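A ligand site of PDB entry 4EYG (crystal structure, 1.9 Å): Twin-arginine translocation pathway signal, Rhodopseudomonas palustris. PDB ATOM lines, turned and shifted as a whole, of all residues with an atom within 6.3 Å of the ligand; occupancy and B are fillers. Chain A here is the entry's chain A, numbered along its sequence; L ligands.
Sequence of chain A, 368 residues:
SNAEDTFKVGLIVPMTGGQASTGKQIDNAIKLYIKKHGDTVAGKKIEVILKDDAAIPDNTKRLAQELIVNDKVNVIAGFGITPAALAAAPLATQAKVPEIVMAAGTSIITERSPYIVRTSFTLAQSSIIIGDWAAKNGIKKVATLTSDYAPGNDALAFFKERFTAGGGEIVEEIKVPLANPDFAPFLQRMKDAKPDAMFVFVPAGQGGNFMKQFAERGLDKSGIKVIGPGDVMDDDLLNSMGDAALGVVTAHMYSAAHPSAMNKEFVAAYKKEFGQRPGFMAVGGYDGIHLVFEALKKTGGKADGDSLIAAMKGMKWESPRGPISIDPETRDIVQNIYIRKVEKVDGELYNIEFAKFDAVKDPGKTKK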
ATOM      1  N   GLN A  19     -15.824  -4.761 -21.783  1.00  0.00           N
ATOM      2  CA  GLN A  19     -16.904  -3.983 -21.151  1.00  0.00           C
ATOM      3  C   GLN A  19     -16.660  -3.720 -19.669  1.00  0.00           C
ATOM      4  O   GLN A  19     -17.606  -3.486 -18.917  1.00  0.00           O
ATOM      5  CB  GLN A  19     -18.276  -4.639 -21.383  1.00  0.00           C
ATOM      6  CG  GLN A  19     -18.786  -4.455 -22.808  1.00  0.00           C
ATOM      7  CD  GLN A  19     -18.059  -5.355 -23.805  1.00  0.00           C
ATOM      8  OE1 GLN A  19     -18.012  -6.571 -23.639  1.00  0.00           O
ATOM      9  NE2 GLN A  19     -17.480  -4.745 -24.852  1.00  0.00           N
ATOM     10  N   THR A  22     -18.371  -0.694 -18.038  1.00  0.00           N
ATOM     11  CA  THR A  22     -19.793  -0.897 -17.684  1.00  0.00           C
ATOM     12  C   THR A  22     -19.936  -1.494 -16.279  1.00  0.00           C
ATOM     13  O   THR A  22     -20.704  -0.995 -15.450  1.00  0.00           O
ATOM     14  CB  THR A  22     -20.513  -1.793 -18.720  1.00  0.00           C
ATOM     15  OG1 THR A  22     -20.544  -1.125 -19.977  1.00  0.00           O
ATOM     16  CG2 THR A  22     -21.951  -2.098 -18.314  1.00  0.00           C
ATOM     17  N   GLY A  80     -24.182  -6.895 -18.560  1.00  0.00           N
ATOM     18  CA  GLY A  80     -23.505  -5.833 -19.289  1.00  0.00           C
ATOM     19  C   GLY A  80     -23.751  -5.815 -20.780  1.00  0.00           C
ATOM     20  O   GLY A  80     -23.666  -4.752 -21.405  1.00  0.00           O
ATOM     21  N   ILE A  81     -24.002  -6.984 -21.356  1.00  0.00           N
ATOM     22  CA  ILE A  81     -24.311  -7.104 -22.778  1.00  0.00           C
ATOM     23  C   ILE A  81     -25.534  -7.988 -22.962  1.00  0.00           C
ATOM     24  O   ILE A  81     -25.882  -8.778 -22.061  1.00  0.00           O
ATOM     25  CB  ILE A  81     -23.103  -7.590 -23.629  1.00  0.00           C
ATOM     26  CG1 ILE A  81     -22.639  -8.995 -23.196  1.00  0.00           C
ATOM     27  CG2 ILE A  81     -21.946  -6.608 -23.524  1.00  0.00           C
ATOM     28  CD1 ILE A  81     -21.776  -9.676 -24.240  1.00  0.00           C
ATOM     29  N   THR A  82     -26.191  -7.851 -24.116  1.00  0.00           N
ATOM     30  CA  THR A  82     -27.397  -8.615 -24.419  1.00  0.00           C
ATOM     31  C   THR A  82     -27.225 -10.141 -24.237  1.00  0.00           C
ATOM     32  O   THR A  82     -28.046 -10.776 -23.552  1.00  0.00           O
ATOM     33  CB  THR A  82     -27.944  -8.232 -25.827  1.00  0.00           C
ATOM     34  OG1 THR A  82     -28.477  -6.907 -25.770  1.00  0.00           O
ATOM     35  CG2 THR A  82     -29.035  -9.216 -26.290  1.00  0.00           C
ATOM     36  N   PRO A  83     -26.152 -10.730 -24.788  1.00  0.00           N
ATOM     37  CA  PRO A  83     -25.977 -12.183 -24.591  1.00  0.00           C
ATOM     38  C   PRO A  83     -25.914 -12.612 -23.115  1.00  0.00           C
ATOM     39  O   PRO A  83     -26.357 -13.721 -22.781  1.00  0.00           O
ATOM     40  CB  PRO A  83     -24.634 -12.452 -25.275  1.00  0.00           C
ATOM     41  CG  PRO A  83     -24.566 -11.438 -26.369  1.00  0.00           C
ATOM     42  CD  PRO A  83     -25.205 -10.193 -25.792  1.00  0.00           C
ATOM     43  N   ALA A 103     -28.019  -2.765 -17.880  1.00  0.00           N
ATOM     44  CA  ALA A 103     -27.157  -2.327 -18.986  1.00  0.00           C
ATOM     45  C   ALA A 103     -27.724  -2.699 -20.349  1.00  0.00           C
ATOM     46  O   ALA A 103     -28.035  -1.816 -21.140  1.00  0.00           O
ATOM     47  CB  ALA A 103     -25.724  -2.883 -18.807  1.00  0.00           C
ATOM     48  N   ALA A 104     -27.879  -4.005 -20.606  1.00  0.00           N
ATOM     49  CA  ALA A 104     -28.216  -4.512 -21.939  1.00  0.00           C
ATOM     50  C   ALA A 104     -29.469  -3.859 -22.573  1.00  0.00           C
ATOM     51  O   ALA A 104     -30.464  -3.649 -21.901  1.00  0.00           O
ATOM     52  CB  ALA A 104     -28.346  -6.035 -21.898  1.00  0.00           C
ATOM     53  N   GLY A 105     -29.397  -3.553 -23.876  1.00  0.00           N
ATOM     54  CA  GLY A 105     -30.403  -2.704 -24.516  1.00  0.00           C
ATOM     55  C   GLY A 105     -31.180  -3.234 -25.716  1.00  0.00           C
ATOM     56  O   GLY A 105     -31.764  -2.460 -26.460  1.00  0.00           O
ATOM     57  N   THR A 106     -31.200  -4.546 -25.909  1.00  0.00           N
ATOM     58  CA  THR A 106     -31.945  -5.127 -27.040  1.00  0.00           C
ATOM     59  C   THR A 106     -33.417  -5.233 -26.653  1.00  0.00           C
ATOM     60  O   THR A 106     -33.737  -5.662 -25.535  1.00  0.00           O
ATOM     61  CB  THR A 106     -31.360  -6.503 -27.411  1.00  0.00           C
ATOM     62  OG1 THR A 106     -30.010  -6.320 -27.844  1.00  0.00           O
ATOM     63  CG2 THR A 106     -32.164  -7.179 -28.524  1.00  0.00           C
ATOM     64  N   ILE A 109     -35.207  -8.549 -24.976  1.00  0.00           N
ATOM     65  CA  ILE A 109     -34.752  -9.119 -23.720  1.00  0.00           C
ATOM     66  C   ILE A 109     -35.881  -9.317 -22.702  1.00  0.00           C
ATOM     67  O   ILE A 109     -35.936 -10.371 -22.080  1.00  0.00           O
ATOM     68  CB  ILE A 109     -33.598  -8.292 -23.084  1.00  0.00           C
ATOM     69  CG1 ILE A 109     -32.320  -8.412 -23.946  1.00  0.00           C
ATOM     70  CG2 ILE A 109     -33.336  -8.761 -21.662  1.00  0.00           C
ATOM     71  CD1 ILE A 109     -31.181  -7.521 -23.503  1.00  0.00           C
ATOM     72  N   PHE A 121     -32.295   0.852 -20.921  1.00  0.00           N
ATOM     73  CA  PHE A 121     -32.825   1.502 -22.129  1.00  0.00           C
ATOM     74  C   PHE A 121     -33.046   0.397 -23.139  1.00  0.00           C
ATOM     75  O   PHE A 121     -32.607  -0.740 -22.914  1.00  0.00           O
ATOM     76  CB  PHE A 121     -31.795   2.509 -22.726  1.00  0.00           C
ATOM     77  CG  PHE A 121     -30.391   1.932 -22.829  1.00  0.00           C
ATOM     78  CD1 PHE A 121     -30.022   1.118 -23.908  1.00  0.00           C
ATOM     79  CD2 PHE A 121     -29.470   2.148 -21.819  1.00  0.00           C
ATOM     80  CE1 PHE A 121     -28.747   0.567 -23.974  1.00  0.00           C
ATOM     81  CE2 PHE A 121     -28.191   1.590 -21.874  1.00  0.00           C
ATOM     82  CZ  PHE A 121     -27.823   0.799 -22.954  1.00  0.00           C
ATOM     83  N   LEU A 123     -32.145   0.247 -27.422  1.00  0.00           N
ATOM     84  CA  LEU A 123     -31.592   1.013 -28.557  1.00  0.00           C
ATOM     85  C   LEU A 123     -32.676   1.667 -29.395  1.00  0.00           C
ATOM     86  O   LEU A 123     -32.491   2.776 -29.898  1.00  0.00           O
ATOM     87  CB  LEU A 123     -30.669   0.159 -29.439  1.00  0.00           C
ATOM     88  CG  LEU A 123     -29.169   0.258 -29.085  1.00  0.00           C
ATOM     89  CD1 LEU A 123     -28.617   1.679 -29.320  1.00  0.00           C
ATOM     90  CD2 LEU A 123     -28.909  -0.174 -27.645  1.00  0.00           C
ATOM     91  N   TYR A 149     -23.895  -7.158 -33.403  1.00  0.00           N
ATOM     92  CA  TYR A 149     -24.676  -8.060 -32.552  1.00  0.00           C
ATOM     93  C   TYR A 149     -26.017  -7.416 -32.235  1.00  0.00           C
ATOM     94  O   TYR A 149     -26.302  -6.325 -32.737  1.00  0.00           O
ATOM     95  CB  TYR A 149     -23.864  -8.542 -31.317  1.00  0.00           C
ATOM     96  CG  TYR A 149     -23.666  -7.545 -30.186  1.00  0.00           C
ATOM     97  CD1 TYR A 149     -24.110  -7.867 -28.896  1.00  0.00           C
ATOM     98  CD2 TYR A 149     -23.031  -6.304 -30.388  1.00  0.00           C
ATOM     99  CE1 TYR A 149     -23.952  -6.980 -27.845  1.00  0.00           C
ATOM    100  CE2 TYR A 149     -22.867  -5.404 -29.340  1.00  0.00           C
ATOM    101  CZ  TYR A 149     -23.326  -5.756 -28.075  1.00  0.00           C
ATOM    102  OH  TYR A 149     -23.185  -4.898 -27.011  1.00  0.00           O
ATOM    103  N   ALA A 150     -26.856  -8.085 -31.452  1.00  0.00           N
ATOM    104  CA  ALA A 150     -28.266  -7.679 -31.287  1.00  0.00           C
ATOM    105  C   ALA A 150     -28.603  -6.171 -31.145  1.00  0.00           C
ATOM    106  O   ALA A 150     -29.454  -5.663 -31.879  1.00  0.00           O
ATOM    107  CB  ALA A 150     -28.936  -8.495 -30.172  1.00  0.00           C
ATOM    108  N   PRO A 151     -27.959  -5.446 -30.192  1.00  0.00           N
ATOM    109  CA  PRO A 151     -28.365  -4.041 -30.017  1.00  0.00           C
ATOM    110  C   PRO A 151     -27.981  -3.150 -31.202  1.00  0.00           C
ATOM    111  O   PRO A 151     -28.688  -2.166 -31.502  1.00  0.00           O
ATOM    112  CB  PRO A 151     -27.624  -3.629 -28.732  1.00  0.00           C
ATOM    113  CG  PRO A 151     -26.443  -4.535 -28.681  1.00  0.00           C
ATOM    114  CD  PRO A 151     -26.954  -5.849 -29.195  1.00  0.00           C
ATOM    115  N   LEU A 178     -18.011  -6.942 -31.947  1.00  0.00           N
ATOM    116  CA  LEU A 178     -18.007  -6.501 -30.542  1.00  0.00           C
ATOM    117  C   LEU A 178     -16.587  -6.501 -29.968  1.00  0.00           C
ATOM    118  O   LEU A 178     -16.153  -5.524 -29.331  1.00  0.00           O
ATOM    119  CB  LEU A 178     -18.912  -7.408 -29.704  1.00  0.00           C
ATOM    120  CG  LEU A 178     -18.974  -7.113 -28.199  1.00  0.00           C
ATOM    121  CD1 LEU A 178     -19.307  -5.646 -27.935  1.00  0.00           C
ATOM    122  CD2 LEU A 178     -19.965  -8.033 -27.484  1.00  0.00           C
ATOM    123  N   PHE A 201     -23.379   3.306 -33.866  1.00  0.00           N
ATOM    124  CA  PHE A 201     -23.558   2.620 -32.592  1.00  0.00           C
ATOM    125  C   PHE A 201     -22.371   1.725 -32.239  1.00  0.00           C
ATOM    126  O   PHE A 201     -22.015   0.799 -32.987  1.00  0.00           O
ATOM    127  CB  PHE A 201     -24.848   1.785 -32.511  1.00  0.00           C
ATOM    128  CG  PHE A 201     -24.867   0.873 -31.309  1.00  0.00           C
ATOM    129  CD1 PHE A 201     -25.122   1.394 -30.044  1.00  0.00           C
ATOM    130  CD2 PHE A 201     -24.508  -0.479 -31.421  1.00  0.00           C
ATOM    131  CE1 PHE A 201     -25.093   0.580 -28.916  1.00  0.00           C
ATOM    132  CE2 PHE A 201     -24.475  -1.289 -30.301  1.00  0.00           C
ATOM    133  CZ  PHE A 201     -24.759  -0.774 -29.057  1.00  0.00           C
ATOM    134  N   VAL A 202     -21.763   2.008 -31.088  1.00  0.00           N
ATOM    135  CA  VAL A 202     -20.811   1.080 -30.459  1.00  0.00           C
ATOM    136  C   VAL A 202     -21.189   1.045 -28.981  1.00  0.00           C
ATOM    137  O   VAL A 202     -21.753   2.016 -28.487  1.00  0.00           O
ATOM    138  CB  VAL A 202     -19.337   1.546 -30.620  1.00  0.00           C
ATOM    139  CG1 VAL A 202     -18.910   1.484 -32.093  1.00  0.00           C
ATOM    140  CG2 VAL A 202     -19.141   2.950 -30.058  1.00  0.00           C
ATOM    141  N   PRO A 203     -20.900  -0.069 -28.273  1.00  0.00           N
ATOM    142  CA  PRO A 203     -21.323  -0.159 -26.864  1.00  0.00           C
ATOM    143  C   PRO A 203     -20.563   0.805 -25.946  1.00  0.00           C
ATOM    144  O   PRO A 203     -19.487   1.271 -26.309  1.00  0.00           O
ATOM    145  CB  PRO A 203     -20.960  -1.606 -26.486  1.00  0.00           C
ATOM    146  CG  PRO A 203     -19.850  -1.961 -27.418  1.00  0.00           C
ATOM    147  CD  PRO A 203     -20.249  -1.310 -28.726  1.00  0.00           C
ATOM    148  N   ALA A 204     -21.109   1.086 -24.764  1.00  0.00           N
ATOM    149  CA  ALA A 204     -20.367   1.795 -23.722  1.00  0.00           C
ATOM    150  C   ALA A 204     -18.927   1.272 -23.674  1.00  0.00           C
ATOM    151  O   ALA A 204     -18.681   0.053 -23.735  1.00  0.00           O
ATOM    152  CB  ALA A 204     -21.038   1.618 -22.367  1.00  0.00           C
ATOM    153  N   GLY A 205     -17.964   2.186 -23.593  1.00  0.00           N
ATOM    154  CA  GLY A 205     -16.553   1.821 -23.443  1.00  0.00           C
ATOM    155  C   GLY A 205     -15.746   1.917 -24.733  1.00  0.00           C
ATOM    156  O   GLY A 205     -14.522   1.953 -24.667  1.00  0.00           O
ATOM    157  N   ASP A 231     -24.694   6.059 -26.956  1.00  0.00           N
ATOM    158  CA  ASP A 231     -23.669   5.122 -26.467  1.00  0.00           C
ATOM    159  C   ASP A 231     -22.271   5.540 -26.852  1.00  0.00           C
ATOM    160  O   ASP A 231     -21.359   5.473 -26.018  1.00  0.00           O
ATOM    161  CB  ASP A 231     -23.956   3.681 -26.924  1.00  0.00           C
ATOM    162  CG  ASP A 231     -25.380   3.256 -26.635  1.00  0.00           C
ATOM    163  OD1 ASP A 231     -25.584   2.400 -25.731  1.00  0.00           O
ATOM    164  OD2 ASP A 231     -26.301   3.808 -27.287  1.00  0.00           O
ATOM    165  N   HIS A 252     -30.336  10.157 -26.359  1.00  0.00           N
ATOM    166  CA  HIS A 252     -30.134   9.196 -25.279  1.00  0.00           C
ATOM    167  C   HIS A 252     -30.985   9.460 -24.072  1.00  0.00           C
ATOM    168  O   HIS A 252     -31.580  10.539 -23.950  1.00  0.00           O
ATOM    169  CB  HIS A 252     -28.651   9.137 -24.877  1.00  0.00           C
ATOM    170  CG  HIS A 252     -28.150   7.728 -24.639  1.00  0.00           C
ATOM    171  ND1 HIS A 252     -27.013   7.468 -23.949  1.00  0.00           N
ATOM    172  CD2 HIS A 252     -28.664   6.489 -25.027  1.00  0.00           C
ATOM    173  CE1 HIS A 252     -26.811   6.131 -23.905  1.00  0.00           C
ATOM    174  NE2 HIS A 252     -27.839   5.529 -24.554  1.00  0.00           N
ATOM    175  N   PHE A 280     -24.018   6.773 -18.524  1.00  0.00           N
ATOM    176  CA  PHE A 280     -25.363   6.219 -18.586  1.00  0.00           C
ATOM    177  C   PHE A 280     -25.453   4.788 -18.001  1.00  0.00           C
ATOM    178  O   PHE A 280     -26.512   4.378 -17.560  1.00  0.00           O
ATOM    179  CB  PHE A 280     -25.901   6.288 -20.010  1.00  0.00           C
ATOM    180  CG  PHE A 280     -25.181   5.400 -21.005  1.00  0.00           C
ATOM    181  CD1 PHE A 280     -25.646   4.113 -21.273  1.00  0.00           C
ATOM    182  CD2 PHE A 280     -24.083   5.870 -21.722  1.00  0.00           C
ATOM    183  CE1 PHE A 280     -25.012   3.289 -22.210  1.00  0.00           C
ATOM    184  CE2 PHE A 280     -23.441   5.067 -22.657  1.00  0.00           C
ATOM    185  CZ  PHE A 280     -23.903   3.772 -22.914  1.00  0.00           C
ATOM    186  N   MET A 281     -24.349   4.063 -17.966  1.00  0.00           N
ATOM    187  CA  MET A 281     -24.367   2.742 -17.293  1.00  0.00           C
ATOM    188  C   MET A 281     -24.466   2.857 -15.775  1.00  0.00           C
ATOM    189  O   MET A 281     -25.130   2.022 -15.125  1.00  0.00           O
ATOM    190  CB  MET A 281     -23.158   1.896 -17.705  1.00  0.00           C
ATOM    191  CG  MET A 281     -23.204   1.475 -19.188  1.00  0.00           C
ATOM    192  SD  MET A 281     -24.889   0.535 -19.615  1.00  0.00           S
ATOM    193  CE  MET A 281     -24.294  -0.314 -21.240  1.00  0.00           C
HETATM  194  C1  LIG L   1     -25.541  -3.127 -25.076  1.00  0.00           C
HETATM  195  C2  LIG L   1     -26.263  -2.042 -25.588  1.00  0.00           C
HETATM  196  C3  LIG L   1     -24.284  -2.943 -24.442  1.00  0.00           C
HETATM  197  C4  LIG L   1     -25.752  -0.728 -25.470  1.00  0.00           C
HETATM  198  C5  LIG L   1     -23.750  -1.661 -24.300  1.00  0.00           C
HETATM  199  O1  LIG L   1     -22.553  -1.393 -23.684  1.00  0.00           O
HETATM  200  C6  LIG L   1     -24.522  -0.508 -24.846  1.00  0.00           C
HETATM  201  C7  LIG L   1     -26.084  -4.520 -25.229  1.00  0.00           C
HETATM  202  C8  LIG L   1     -21.787  -2.407 -22.995  1.00  0.00           C
HETATM  203  O2  LIG L   1     -27.316  -4.736 -25.329  1.00  0.00           O
HETATM  204  O3  LIG L   1     -25.260  -5.457 -25.306  1.00  0.00           O
HETATM  205  O4  LIG L   1     -23.995   0.753 -24.708  1.00  0.00           O
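O of Gly 105 is in hydrogen-bond range of N of Leu 123, at 2.9 Å.
The side-chain hydroxyl (OG1) of Thr 82 lies within hydrogen-bond range of the side-chain hydroxyl (OG1) of Thr 106.
O4 of the ligand sits at hydrogen-bond distance from OD1 of Asp 231 (2.5 Å).
An oxygen (O2) of the ligand lies within hydrogen-bond range of the backbone NH (N) of Gly 105, at 2.8 Å.
The side-chain hydroxyl of Thr 82 lies within hydrogen-bond range of an oxygen (O2) of the ligand (2.5 Å).
The backbone NH (N) of Thr 82 sits at hydrogen-bond distance from an oxygen (O3) of the ligand, at 2.8 Å.
OH of Tyr 149 sits at hydrogen-bond distance from O3 of the ligand (2.7 Å).
The backbone NH of Ala 204 lies within hydrogen-bond range of an oxygen (O4) of the ligand (2.9 Å).
Merely in contact with the ligand: Gln 19, Thr 22, Gly 80, Ile 81, Ala 104, Thr 106, Phe 121, Leu 123, Pro 151, Phe 201, Pro 203, Phe 280 and Met 281.
Hydrophobic or aromatic side chains that line the ligand: Ile 81, Ala 104, Phe 121, Leu 123, Tyr 149, Pro 151, Phe 201, Pro 203, Ala 204, Phe 280 and Met 281.
The nearest printed residue that does not touch the ligand is Val 202 (4.6 Å).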
